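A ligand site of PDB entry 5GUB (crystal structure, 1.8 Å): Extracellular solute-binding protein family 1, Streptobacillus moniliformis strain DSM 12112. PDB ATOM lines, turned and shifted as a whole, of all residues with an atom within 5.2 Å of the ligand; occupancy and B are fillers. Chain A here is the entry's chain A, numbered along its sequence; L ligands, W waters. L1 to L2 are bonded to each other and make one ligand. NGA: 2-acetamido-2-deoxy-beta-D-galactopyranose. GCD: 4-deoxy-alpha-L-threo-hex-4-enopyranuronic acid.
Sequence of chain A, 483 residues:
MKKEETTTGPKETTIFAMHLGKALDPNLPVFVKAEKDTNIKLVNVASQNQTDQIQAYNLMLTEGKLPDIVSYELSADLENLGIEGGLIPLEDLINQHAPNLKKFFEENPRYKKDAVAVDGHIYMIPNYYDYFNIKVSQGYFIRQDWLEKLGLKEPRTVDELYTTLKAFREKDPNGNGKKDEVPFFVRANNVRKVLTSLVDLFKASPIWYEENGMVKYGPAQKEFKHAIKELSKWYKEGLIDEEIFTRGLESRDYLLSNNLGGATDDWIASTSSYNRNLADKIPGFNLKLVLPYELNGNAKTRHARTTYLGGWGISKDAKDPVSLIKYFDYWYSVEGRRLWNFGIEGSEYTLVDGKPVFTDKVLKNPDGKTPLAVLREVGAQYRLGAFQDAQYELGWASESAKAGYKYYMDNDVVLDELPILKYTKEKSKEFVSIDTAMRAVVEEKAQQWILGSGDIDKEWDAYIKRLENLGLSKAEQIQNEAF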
ATOM      1  N   HIS A  19     -37.528 -15.718 -10.499  1.00  0.00           N
ATOM      2  CA  HIS A  19     -36.308 -14.952 -10.326  1.00  0.00           C
ATOM      3  C   HIS A  19     -35.161 -15.896 -10.041  1.00  0.00           C
ATOM      4  O   HIS A  19     -35.284 -16.794  -9.222  1.00  0.00           O
ATOM      5  CB  HIS A  19     -36.437 -13.933  -9.186  1.00  0.00           C
ATOM      6  CG  HIS A  19     -35.245 -13.033  -9.067  1.00  0.00           C
ATOM      7  ND1 HIS A  19     -34.682 -12.400 -10.153  1.00  0.00           N
ATOM      8  CD2 HIS A  19     -34.489 -12.677  -7.996  1.00  0.00           C
ATOM      9  CE1 HIS A  19     -33.635 -11.701  -9.767  1.00  0.00           C
ATOM     10  NE2 HIS A  19     -33.488 -11.856  -8.458  1.00  0.00           N
ATOM     11  N   LEU A  20     -34.047 -15.684 -10.731  1.00  0.00           N
ATOM     12  CA  LEU A  20     -32.849 -16.508 -10.572  1.00  0.00           C
ATOM     13  C   LEU A  20     -33.199 -17.993 -10.653  1.00  0.00           C
ATOM     14  O   LEU A  20     -32.722 -18.817  -9.847  1.00  0.00           O
ATOM     15  CB  LEU A  20     -32.148 -16.162  -9.250  1.00  0.00           C
ATOM     16  CG  LEU A  20     -31.546 -14.748  -9.250  1.00  0.00           C
ATOM     17  CD1 LEU A  20     -31.040 -14.360  -7.867  1.00  0.00           C
ATOM     18  CD2 LEU A  20     -30.384 -14.690 -10.266  1.00  0.00           C
ATOM     19  N   GLU A  73     -38.490 -10.184 -16.045  1.00  0.00           N
ATOM     20  CA  GLU A  73     -37.193  -9.526 -15.988  1.00  0.00           C
ATOM     21  C   GLU A  73     -36.939  -8.642 -17.214  1.00  0.00           C
ATOM     22  O   GLU A  73     -36.146  -7.695 -17.144  1.00  0.00           O
ATOM     23  CB  GLU A  73     -36.067 -10.554 -15.817  1.00  0.00           C
ATOM     24  CG  GLU A  73     -34.690  -9.897 -15.560  1.00  0.00           C
ATOM     25  CD  GLU A  73     -33.617 -10.848 -15.036  1.00  0.00           C
ATOM     26  OE1 GLU A  73     -33.887 -11.618 -14.088  1.00  0.00           O
ATOM     27  OE2 GLU A  73     -32.492 -10.828 -15.588  1.00  0.00           O
ATOM     28  N   ASN A 127     -38.412  -2.995 -10.653  1.00  0.00           N
ATOM     29  CA  ASN A 127     -37.683  -3.319  -9.439  1.00  0.00           C
ATOM     30  C   ASN A 127     -36.419  -2.460  -9.401  1.00  0.00           C
ATOM     31  O   ASN A 127     -35.480  -2.722 -10.135  1.00  0.00           O
ATOM     32  CB  ASN A 127     -37.337  -4.808  -9.385  1.00  0.00           C
ATOM     33  CG  ASN A 127     -37.075  -5.278  -7.970  1.00  0.00           C
ATOM     34  OD1 ASN A 127     -38.001  -5.703  -7.268  1.00  0.00           O
ATOM     35  ND2 ASN A 127     -35.817  -5.205  -7.537  1.00  0.00           N
ATOM     36  N   TYR A 129     -32.962  -0.787  -8.228  1.00  0.00           N
ATOM     37  CA  TYR A 129     -31.772  -0.812  -7.402  1.00  0.00           C
ATOM     38  C   TYR A 129     -31.698   0.497  -6.618  1.00  0.00           C
ATOM     39  O   TYR A 129     -32.416   1.453  -6.950  1.00  0.00           O
ATOM     40  CB  TYR A 129     -30.510  -0.992  -8.259  1.00  0.00           C
ATOM     41  CG  TYR A 129     -30.303  -2.392  -8.814  1.00  0.00           C
ATOM     42  CD1 TYR A 129     -29.985  -3.455  -7.967  1.00  0.00           C
ATOM     43  CD2 TYR A 129     -30.383  -2.642 -10.182  1.00  0.00           C
ATOM     44  CE1 TYR A 129     -29.782  -4.735  -8.470  1.00  0.00           C
ATOM     45  CE2 TYR A 129     -30.179  -3.922 -10.685  1.00  0.00           C
ATOM     46  CZ  TYR A 129     -29.877  -4.962  -9.826  1.00  0.00           C
ATOM     47  OH  TYR A 129     -29.661  -6.237 -10.332  1.00  0.00           O
ATOM     48  N   ARG A 187     -20.551 -17.011 -12.917  1.00  0.00           N
ATOM     49  CA  ARG A 187     -21.765 -17.418 -12.219  1.00  0.00           C
ATOM     50  C   ARG A 187     -22.976 -16.896 -12.976  1.00  0.00           C
ATOM     51  O   ARG A 187     -23.111 -15.688 -13.185  1.00  0.00           O
ATOM     52  CB  ARG A 187     -21.758 -16.916 -10.772  1.00  0.00           C
ATOM     53  CG  ARG A 187     -22.979 -17.362  -9.944  1.00  0.00           C
ATOM     54  CD  ARG A 187     -22.797 -16.906  -8.489  1.00  0.00           C
ATOM     55  NE  ARG A 187     -22.770 -15.441  -8.392  1.00  0.00           N
ATOM     56  CZ  ARG A 187     -23.785 -14.678  -7.979  1.00  0.00           C
ATOM     57  NH1 ARG A 187     -24.930 -15.220  -7.551  1.00  0.00           N
ATOM     58  NH2 ARG A 187     -23.637 -13.367  -7.943  1.00  0.00           N
ATOM     59  N   ASN A 189     -27.184 -18.001 -14.791  1.00  0.00           N
ATOM     60  CA  ASN A 189     -28.277 -18.941 -15.037  1.00  0.00           C
ATOM     61  C   ASN A 189     -28.847 -18.834 -16.437  1.00  0.00           C
ATOM     62  O   ASN A 189     -29.890 -19.406 -16.731  1.00  0.00           O
ATOM     63  CB  ASN A 189     -29.393 -18.757 -13.995  1.00  0.00           C
ATOM     64  CG  ASN A 189     -30.080 -17.415 -14.093  1.00  0.00           C
ATOM     65  OD1 ASN A 189     -29.426 -16.374 -14.123  1.00  0.00           O
ATOM     66  ND2 ASN A 189     -31.416 -17.443 -14.135  1.00  0.00           N
ATOM     67  N   LYS A 193     -25.896 -14.281 -19.412  1.00  0.00           N
ATOM     68  CA  LYS A 193     -25.089 -13.956 -18.226  1.00  0.00           C
ATOM     69  C   LYS A 193     -23.692 -14.586 -18.287  1.00  0.00           C
ATOM     70  O   LYS A 193     -22.727 -14.007 -17.774  1.00  0.00           O
ATOM     71  CB  LYS A 193     -25.798 -14.394 -16.943  1.00  0.00           C
ATOM     72  CG  LYS A 193     -26.858 -13.410 -16.493  1.00  0.00           C
ATOM     73  CD  LYS A 193     -27.442 -13.820 -15.136  1.00  0.00           C
ATOM     74  CE  LYS A 193     -28.451 -12.792 -14.653  1.00  0.00           C
ATOM     75  NZ  LYS A 193     -29.007 -13.153 -13.321  1.00  0.00           N
ATOM     76  N   LEU A 249     -25.985 -21.515 -11.193  1.00  0.00           N
ATOM     77  CA  LEU A 249     -25.747 -20.482 -10.188  1.00  0.00           C
ATOM     78  C   LEU A 249     -24.948 -20.962  -8.976  1.00  0.00           C
ATOM     79  O   LEU A 249     -24.448 -20.143  -8.216  1.00  0.00           O
ATOM     80  CB  LEU A 249     -27.080 -19.890  -9.731  1.00  0.00           C
ATOM     81  CG  LEU A 249     -27.727 -19.006 -10.797  1.00  0.00           C
ATOM     82  CD1 LEU A 249     -29.154 -18.627 -10.412  1.00  0.00           C
ATOM     83  CD2 LEU A 249     -26.901 -17.740 -11.006  1.00  0.00           C
ATOM     84  N   ARG A 252     -19.924 -20.593  -8.351  1.00  0.00           N
ATOM     85  CA  ARG A 252     -18.991 -19.898  -7.483  1.00  0.00           C
ATOM     86  C   ARG A 252     -18.874 -20.608  -6.136  1.00  0.00           C
ATOM     87  O   ARG A 252     -17.756 -20.845  -5.650  1.00  0.00           O
ATOM     88  CB  ARG A 252     -19.439 -18.446  -7.305  1.00  0.00           C
ATOM     89  CG  ARG A 252     -18.513 -17.594  -6.434  1.00  0.00           C
ATOM     90  CD  ARG A 252     -19.108 -16.196  -6.305  1.00  0.00           C
ATOM     91  NE  ARG A 252     -20.439 -16.247  -5.679  1.00  0.00           N
ATOM     92  CZ  ARG A 252     -21.182 -15.172  -5.457  1.00  0.00           C
ATOM     93  NH1 ARG A 252     -20.725 -13.982  -5.823  1.00  0.00           N
ATOM     94  NH2 ARG A 252     -22.377 -15.275  -4.863  1.00  0.00           N
ATOM     95  N   TRP A 267     -20.383 -10.016  -8.944  1.00  0.00           N
ATOM     96  CA  TRP A 267     -20.831  -8.921  -8.091  1.00  0.00           C
ATOM     97  C   TRP A 267     -19.910  -8.700  -6.890  1.00  0.00           C
ATOM     98  O   TRP A 267     -19.474  -9.658  -6.241  1.00  0.00           O
ATOM     99  CB  TRP A 267     -22.243  -9.205  -7.617  1.00  0.00           C
ATOM    100  CG  TRP A 267     -23.256  -9.040  -8.694  1.00  0.00           C
ATOM    101  CD1 TRP A 267     -23.524  -9.900  -9.727  1.00  0.00           C
ATOM    102  CD2 TRP A 267     -24.145  -7.937  -8.827  1.00  0.00           C
ATOM    103  NE1 TRP A 267     -24.546  -9.385 -10.506  1.00  0.00           N
ATOM    104  CE2 TRP A 267     -24.941  -8.176  -9.977  1.00  0.00           C
ATOM    105  CE3 TRP A 267     -24.341  -6.753  -8.111  1.00  0.00           C
ATOM    106  CZ2 TRP A 267     -25.917  -7.283 -10.408  1.00  0.00           C
ATOM    107  CZ3 TRP A 267     -25.319  -5.868  -8.538  1.00  0.00           C
ATOM    108  CH2 TRP A 267     -26.093  -6.133  -9.675  1.00  0.00           C
ATOM    109  N   ILE A 268     -19.621  -7.441  -6.598  1.00  0.00           N
ATOM    110  CA  ILE A 268     -18.545  -7.161  -5.662  1.00  0.00           C
ATOM    111  C   ILE A 268     -18.851  -7.625  -4.217  1.00  0.00           C
ATOM    112  O   ILE A 268     -18.015  -8.301  -3.589  1.00  0.00           O
ATOM    113  CB  ILE A 268     -18.195  -5.654  -5.702  1.00  0.00           C
ATOM    114  CG1 ILE A 268     -17.390  -5.356  -6.986  1.00  0.00           C
ATOM    115  CG2 ILE A 268     -17.366  -5.272  -4.478  1.00  0.00           C
ATOM    116  CD1 ILE A 268     -17.226  -3.887  -7.305  1.00  0.00           C
ATOM    117  N   ALA A 269     -20.032  -7.316  -3.703  1.00  0.00           N
ATOM    118  CA  ALA A 269     -20.296  -7.648  -2.290  1.00  0.00           C
ATOM    119  C   ALA A 269     -20.357  -9.150  -2.034  1.00  0.00           C
ATOM    120  O   ALA A 269     -19.697  -9.628  -1.132  1.00  0.00           O
ATOM    121  CB  ALA A 269     -21.571  -6.980  -1.781  1.00  0.00           C
ATOM    122  N   SER A 270     -21.146  -9.885  -2.808  1.00  0.00           N
ATOM    123  CA  SER A 270     -21.261 -11.316  -2.541  1.00  0.00           C
ATOM    124  C   SER A 270     -19.947 -12.042  -2.832  1.00  0.00           C
ATOM    125  O   SER A 270     -19.620 -13.005  -2.156  1.00  0.00           O
ATOM    126  CB  SER A 270     -22.415 -11.949  -3.348  1.00  0.00           C
ATOM    127  OG  SER A 270     -22.236 -11.826  -4.746  1.00  0.00           O
ATOM    128  N   THR A 271     -19.188 -11.598  -3.830  1.00  0.00           N
ATOM    129  CA  THR A 271     -17.944 -12.276  -4.121  1.00  0.00           C
ATOM    130  C   THR A 271     -16.908 -11.997  -3.028  1.00  0.00           C
ATOM    131  O   THR A 271     -16.068 -12.838  -2.732  1.00  0.00           O
ATOM    132  CB  THR A 271     -17.402 -11.880  -5.514  1.00  0.00           C
ATOM    133  OG1 THR A 271     -18.416 -12.145  -6.492  1.00  0.00           O
ATOM    134  CG2 THR A 271     -16.158 -12.696  -5.871  1.00  0.00           C
ATOM    135  N   ARG A 305     -24.198  -1.129 -12.306  1.00  0.00           N
ATOM    136  CA  ARG A 305     -25.574  -1.353 -11.895  1.00  0.00           C
ATOM    137  C   ARG A 305     -26.492  -0.484 -12.760  1.00  0.00           C
ATOM    138  O   ARG A 305     -26.136   0.639 -13.147  1.00  0.00           O
ATOM    139  CB  ARG A 305     -25.729  -1.061 -10.399  1.00  0.00           C
ATOM    140  CG  ARG A 305     -26.791  -1.885  -9.701  1.00  0.00           C
ATOM    141  CD  ARG A 305     -26.734  -1.683  -8.186  1.00  0.00           C
ATOM    142  NE  ARG A 305     -25.526  -2.252  -7.595  1.00  0.00           N
ATOM    143  CZ  ARG A 305     -25.470  -2.843  -6.406  1.00  0.00           C
ATOM    144  NH1 ARG A 305     -26.571  -2.953  -5.666  1.00  0.00           N
ATOM    145  NH2 ARG A 305     -24.325  -3.324  -5.946  1.00  0.00           N
ATOM    146  N   LEU A 309     -34.220  -3.326 -12.632  1.00  0.00           N
ATOM    147  CA  LEU A 309     -34.202  -4.584 -13.365  1.00  0.00           C
ATOM    148  C   LEU A 309     -35.609  -5.169 -13.378  1.00  0.00           C
ATOM    149  O   LEU A 309     -36.145  -5.507 -12.314  1.00  0.00           O
ATOM    150  CB  LEU A 309     -33.240  -5.572 -12.710  1.00  0.00           C
ATOM    151  CG  LEU A 309     -33.239  -6.997 -13.272  1.00  0.00           C
ATOM    152  CD1 LEU A 309     -32.596  -6.971 -14.653  1.00  0.00           C
ATOM    153  CD2 LEU A 309     -32.518  -7.974 -12.340  1.00  0.00           C
ATOM    154  N   LEU A 372     -26.176 -13.030   1.362  1.00  0.00           N
ATOM    155  CA  LEU A 372     -27.244 -12.791   0.395  1.00  0.00           C
ATOM    156  C   LEU A 372     -27.994 -14.081   0.114  1.00  0.00           C
ATOM    157  O   LEU A 372     -29.213 -14.064  -0.085  1.00  0.00           O
ATOM    158  CB  LEU A 372     -26.679 -12.209  -0.911  1.00  0.00           C
ATOM    159  CG  LEU A 372     -27.681 -11.998  -2.055  1.00  0.00           C
ATOM    160  CD1 LEU A 372     -28.897 -11.254  -1.585  1.00  0.00           C
ATOM    161  CD2 LEU A 372     -27.007 -11.228  -3.210  1.00  0.00           C
ATOM    162  N   ARG A 376     -32.002 -14.523   0.420  1.00  0.00           N
ATOM    163  CA  ARG A 376     -32.856 -14.971  -0.671  1.00  0.00           C
ATOM    164  C   ARG A 376     -33.675 -16.193  -0.250  1.00  0.00           C
ATOM    165  O   ARG A 376     -34.793 -16.371  -0.700  1.00  0.00           O
ATOM    166  CB  ARG A 376     -32.041 -15.310  -1.933  1.00  0.00           C
ATOM    167  CG  ARG A 376     -31.420 -14.076  -2.590  1.00  0.00           C
ATOM    168  CD  ARG A 376     -30.963 -14.382  -4.018  1.00  0.00           C
ATOM    169  NE  ARG A 376     -30.296 -13.218  -4.620  1.00  0.00           N
ATOM    170  CZ  ARG A 376     -30.948 -12.166  -5.089  1.00  0.00           C
ATOM    171  NH1 ARG A 376     -32.285 -12.130  -5.050  1.00  0.00           N
ATOM    172  NH2 ARG A 376     -30.279 -11.140  -5.612  1.00  0.00           N
ATOM    173  N   GLN A 381     -35.133  -9.803  -1.197  1.00  0.00           N
ATOM    174  CA  GLN A 381     -34.445  -9.458  -2.445  1.00  0.00           C
ATOM    175  C   GLN A 381     -35.012 -10.167  -3.670  1.00  0.00           C
ATOM    176  O   GLN A 381     -34.366 -10.239  -4.725  1.00  0.00           O
ATOM    177  CB  GLN A 381     -32.935  -9.771  -2.329  1.00  0.00           C
ATOM    178  CG  GLN A 381     -32.223  -8.947  -1.241  1.00  0.00           C
ATOM    179  CD  GLN A 381     -32.295  -7.452  -1.536  1.00  0.00           C
ATOM    180  OE1 GLN A 381     -32.156  -7.040  -2.685  1.00  0.00           O
ATOM    181  NE2 GLN A 381     -32.516  -6.651  -0.499  1.00  0.00           N
ATOM    182  N   ARG A 383     -36.784 -10.315  -6.873  1.00  0.00           N
ATOM    183  CA  ARG A 383     -37.079  -9.324  -7.897  1.00  0.00           C
ATOM    184  C   ARG A 383     -38.555  -9.335  -8.289  1.00  0.00           C
ATOM    185  O   ARG A 383     -39.049 -10.320  -8.813  1.00  0.00           O
ATOM    186  CB  ARG A 383     -36.201  -9.575  -9.125  1.00  0.00           C
ATOM    187  CG  ARG A 383     -35.996  -8.359 -10.023  1.00  0.00           C
ATOM    188  CD  ARG A 383     -37.133  -8.146 -10.998  1.00  0.00           C
ATOM    189  NE  ARG A 383     -37.505  -9.347 -11.752  1.00  0.00           N
ATOM    190  CZ  ARG A 383     -38.745  -9.598 -12.153  1.00  0.00           C
ATOM    191  NH1 ARG A 383     -39.706  -8.713 -11.879  1.00  0.00           N
ATOM    192  NH2 ARG A 383     -39.051 -10.718 -12.815  1.00  0.00           N
ATOM    193  N   GLN A 388     -34.992  -1.425  -3.820  1.00  0.00           N
ATOM    194  CA  GLN A 388     -33.875  -1.838  -2.981  1.00  0.00           C
ATOM    195  C   GLN A 388     -33.358  -0.692  -2.091  1.00  0.00           C
ATOM    196  O   GLN A 388     -33.433   0.479  -2.451  1.00  0.00           O
ATOM    197  CB  GLN A 388     -32.737  -2.377  -3.850  1.00  0.00           C
ATOM    198  CG  GLN A 388     -31.611  -3.039  -3.079  1.00  0.00           C
ATOM    199  CD  GLN A 388     -30.569  -3.614  -4.018  1.00  0.00           C
ATOM    200  OE1 GLN A 388     -29.760  -2.883  -4.588  1.00  0.00           O
ATOM    201  NE2 GLN A 388     -30.603  -4.922  -4.202  1.00  0.00           N
ATOM    202  N   TYR A 392     -29.322  -2.331   3.237  1.00  0.00           N
ATOM    203  CA  TYR A 392     -29.364  -3.793   3.350  1.00  0.00           C
ATOM    204  C   TYR A 392     -28.012  -4.353   2.900  1.00  0.00           C
ATOM    205  O   TYR A 392     -27.463  -5.254   3.530  1.00  0.00           O
ATOM    206  CB  TYR A 392     -30.538  -4.397   2.519  1.00  0.00           C
ATOM    207  CG  TYR A 392     -30.071  -5.275   1.359  1.00  0.00           C
ATOM    208  CD1 TYR A 392     -29.809  -4.733   0.111  1.00  0.00           C
ATOM    209  CD2 TYR A 392     -29.875  -6.645   1.546  1.00  0.00           C
ATOM    210  CE1 TYR A 392     -29.344  -5.535  -0.942  1.00  0.00           C
ATOM    211  CE2 TYR A 392     -29.414  -7.451   0.507  1.00  0.00           C
ATOM    212  CZ  TYR A 392     -29.145  -6.883  -0.732  1.00  0.00           C
ATOM    213  OH  TYR A 392     -28.689  -7.701  -1.754  1.00  0.00           O
ATOM    214  N   GLU A 393     -27.478  -3.819   1.806  1.00  0.00           N
ATOM    215  CA  GLU A 393     -26.240  -4.349   1.242  1.00  0.00           C
ATOM    216  C   GLU A 393     -25.067  -3.974   2.130  1.00  0.00           C
ATOM    217  O   GLU A 393     -24.226  -4.806   2.444  1.00  0.00           O
ATOM    218  CB  GLU A 393     -26.044  -3.829  -0.194  1.00  0.00           C
ATOM    219  CG  GLU A 393     -24.870  -4.451  -0.968  1.00  0.00           C
ATOM    220  CD  GLU A 393     -24.943  -4.197  -2.471  1.00  0.00           C
ATOM    221  OE1 GLU A 393     -23.899  -4.262  -3.158  1.00  0.00           O
ATOM    222  OE2 GLU A 393     -26.049  -3.967  -2.987  1.00  0.00           O
ATOM    223  N   TRP A 396     -24.442  -6.248   5.244  1.00  0.00           N
ATOM    224  CA  TRP A 396     -23.704  -7.523   5.253  1.00  0.00           C
ATOM    225  C   TRP A 396     -22.391  -7.463   4.467  1.00  0.00           C
ATOM    226  O   TRP A 396     -21.557  -8.355   4.610  1.00  0.00           O
ATOM    227  CB  TRP A 396     -24.570  -8.671   4.727  1.00  0.00           C
ATOM    228  CG  TRP A 396     -25.128  -8.480   3.341  1.00  0.00           C
ATOM    229  CD1 TRP A 396     -26.355  -7.973   3.014  1.00  0.00           C
ATOM    230  CD2 TRP A 396     -24.496  -8.831   2.088  1.00  0.00           C
ATOM    231  NE1 TRP A 396     -26.515  -7.958   1.651  1.00  0.00           N
ATOM    232  CE2 TRP A 396     -25.395  -8.471   1.059  1.00  0.00           C
ATOM    233  CE3 TRP A 396     -23.262  -9.388   1.749  1.00  0.00           C
ATOM    234  CZ2 TRP A 396     -25.098  -8.686  -0.299  1.00  0.00           C
ATOM    235  CZ3 TRP A 396     -22.963  -9.594   0.387  1.00  0.00           C
ATOM    236  CH2 TRP A 396     -23.886  -9.233  -0.609  1.00  0.00           C
HETATM  237  C1  NGA L   1     -29.618 -10.348 -10.451  1.00  0.00           C
HETATM  238  C2  NGA L   1     -29.725  -9.841  -9.005  1.00  0.00           C
HETATM  239  C3  NGA L   1     -28.352  -9.591  -8.416  1.00  0.00           C
HETATM  240  C4  NGA L   1     -27.493 -10.850  -8.572  1.00  0.00           C
HETATM  241  C5  NGA L   1     -27.519 -11.310 -10.017  1.00  0.00           C
HETATM  242  C6  NGA L   1     -26.712 -12.585 -10.221  1.00  0.00           C
HETATM  243  C7  NGA L   1     -31.673  -8.609  -8.260  1.00  0.00           C
HETATM  244  C8  NGA L   1     -32.443  -7.316  -8.400  1.00  0.00           C
HETATM  245  N2  NGA L   1     -30.535  -8.631  -8.936  1.00  0.00           N
HETATM  246  O1  NGA L   1     -30.913 -10.638 -10.922  1.00  0.00           O
HETATM  247  O3  NGA L   1     -28.554  -9.297  -7.042  1.00  0.00           O
HETATM  248  O4  NGA L   1     -27.956 -11.888  -7.713  1.00  0.00           O
HETATM  249  O5  NGA L   1     -28.859 -11.531 -10.476  1.00  0.00           O
HETATM  250  O6  NGA L   1     -26.744 -12.895 -11.605  1.00  0.00           O
HETATM  251  O7  NGA L   1     -32.071  -9.568  -7.574  1.00  0.00           O
HETATM  252  C1  GCD L   2     -27.576  -8.372  -6.576  1.00  0.00           C
HETATM  253  C2  GCD L   2     -28.175  -7.557  -5.428  1.00  0.00           C
HETATM  254  C3  GCD L   2     -27.140  -6.584  -4.896  1.00  0.00           C
HETATM  255  C4  GCD L   2     -25.830  -7.313  -4.652  1.00  0.00           C
HETATM  256  C5  GCD L   2     -25.556  -8.490  -5.228  1.00  0.00           C
HETATM  257  C6  GCD L   2     -24.312  -9.224  -4.969  1.00  0.00           C
HETATM  258  O2  GCD L   2     -29.322  -6.837  -5.904  1.00  0.00           O
HETATM  259  O3  GCD L   2     -27.595  -6.056  -3.633  1.00  0.00           O
HETATM  260  O5  GCD L   2     -26.468  -9.131  -6.135  1.00  0.00           O
HETATM  261  O6A GCD L   2     -23.392  -8.672  -4.330  1.00  0.00           O
HETATM  262  O6B GCD L   2     -24.222 -10.394  -5.401  1.00  0.00           O
HETATM  263  O   HOH W   1     -24.442 -13.987 -12.001  1.00  0.00           O
HETATM  264  O   HOH W   2     -30.758 -10.851 -13.492  1.00  0.00           O
HETATM  265  O   HOH W   3     -25.826 -10.640 -12.754  1.00  0.00           O
HETATM  266  O   HOH W   4     -22.483  -6.117  -4.713  1.00  0.00           O
HETATM  267  O   HOH W   5     -34.402  -8.310  -6.390  1.00  0.00           O
HETATM  268  O   HOH W   6     -31.648  -8.029  -5.105  1.00  0.00           O
HETATM  269  O   HOH W   7     -33.410  -4.290  -8.959  1.00  0.00           O
HETATM  270  O   HOH W   8     -25.754 -12.425  -6.275  1.00  0.00           O
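An oxygen (O6A) of GCD L2 sits at hydrogen-bond distance from the backbone NH (N) of Ser 270, at 3.0 Å.
An oxygen (O6B) of GCD L2 is in hydrogen-bond range of the side-chain hydroxyl of Ser 270, 2.5 Å away.
O3 of GCD L2 sits at hydrogen-bond distance from OE2 of Glu 393, 2.7 Å away.
O3 of GCD L2 sits at hydrogen-bond distance from OH of Tyr 392.
A ring nitrogen (NE2) of His 19 lies within hydrogen-bond range of an oxygen (O7) of NGA L1 (2.8 Å).
NZ of Lys 193 lies within hydrogen-bond range of O6 of NGA L1, 2.9 Å away.
An oxygen (O2) of GCD L2 is in hydrogen-bond range of the side-chain amide nitrogen (NE2) of Gln 388 (2.9 Å).
The guanidinium group (NH2) of Arg 376 lies within hydrogen-bond range of an oxygen (O3) of NGA L1, 2.9 Å away.
OH of Tyr 129 is in hydrogen-bond range of N2 of NGA L1, at 2.9 Å.
An oxygen (O6B) of GCD L2 is in salt-bridge range of the guanidinium group (NH2) of Arg 187, at 3.96 Å.
The side-chain hydroxyl (OG) of Ser 270 is in hydrogen-bond range of the guanidinium group (NH1) of Arg 252, at 2.8 Å.
NE1 of Trp 396 sits close to O of Tyr 392.
The side-chain amino group (NZ) of Lys 193 is in hydrogen-bond range of the side-chain amide oxygen (OD1) of Asn 189 (3.3 Å).
The side-chain amide oxygen (OE1) of Gln 381 is in hydrogen-bond range of the side-chain amide nitrogen (NE2) of Gln 388 (3.0 Å).
The guanidinium group (NH1) of Arg 305 is in hydrogen-bond range of the side-chain amide oxygen (OE1) of Gln 388 (3.4 Å).
O of Gln 381 is in hydrogen-bond range of NH1 of Arg 376 (2.8 Å).
The side-chain hydroxyl (OG1) of Thr 271 is in hydrogen-bond range of the backbone carbonyl oxygen (O) of Trp 267, 2.7 Å away.
The backbone carbonyl oxygen (O) of Asn 127 sits at hydrogen-bond distance from the backbone NH (N) of Leu 309 (2.9 Å).
Residues that only touch the ligand: Leu 20 (3.5 Å), Trp 267 (3.2 Å), Ala 269 (3.6 Å), Arg 305 (3.8 Å), Leu 309 (3.4 Å), Leu 372 (3.6 Å), Gln 381 (3.7 Å) and Trp 396 (3.8 Å).
Hydrophobic or aromatic side chains that line the ligand: His 19, Leu 20, Tyr 129, Trp 267, Ala 269, Leu 309, Leu 372, Tyr 392 and Trp 396.
Within 4 Å of the ligand: His 19, Leu 20, Tyr 129, Arg 187, Lys 193, Trp 267, Ala 269, Ser 270, Arg 305, Leu 309, Leu 372, Arg 376, Gln 381, Gln 388, Tyr 392, Glu 393 and Trp 396.
Water W1 lies within hydrogen-bond range of O of Arg 187 (2.5 Å) and O6 of NGA L1 (2.6 Å).
Water W2 lies within hydrogen-bond range of O1 of NGA L1 (2.6 Å), OE2 of Glu 73 (2.7 Å) and NZ of Lys 193 (2.9 Å).
Water W8 bridges O4 of NGA L1 and NH2 of Arg 187.
Water W6 lies within hydrogen-bond range of the side-chain amide oxygen of Gln 381, an oxygen (O2) of GCD L2, the side-chain amide nitrogen of Gln 388 and the guanidinium group of Arg 376.
Water W4 lies within hydrogen-bond range of O6A of GCD L2, OE1 of Glu 393 and N of Ala 269.
Water W5 lies within hydrogen-bond range of O of Gln 381, O7 of NGA L1 and N of Arg 383.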
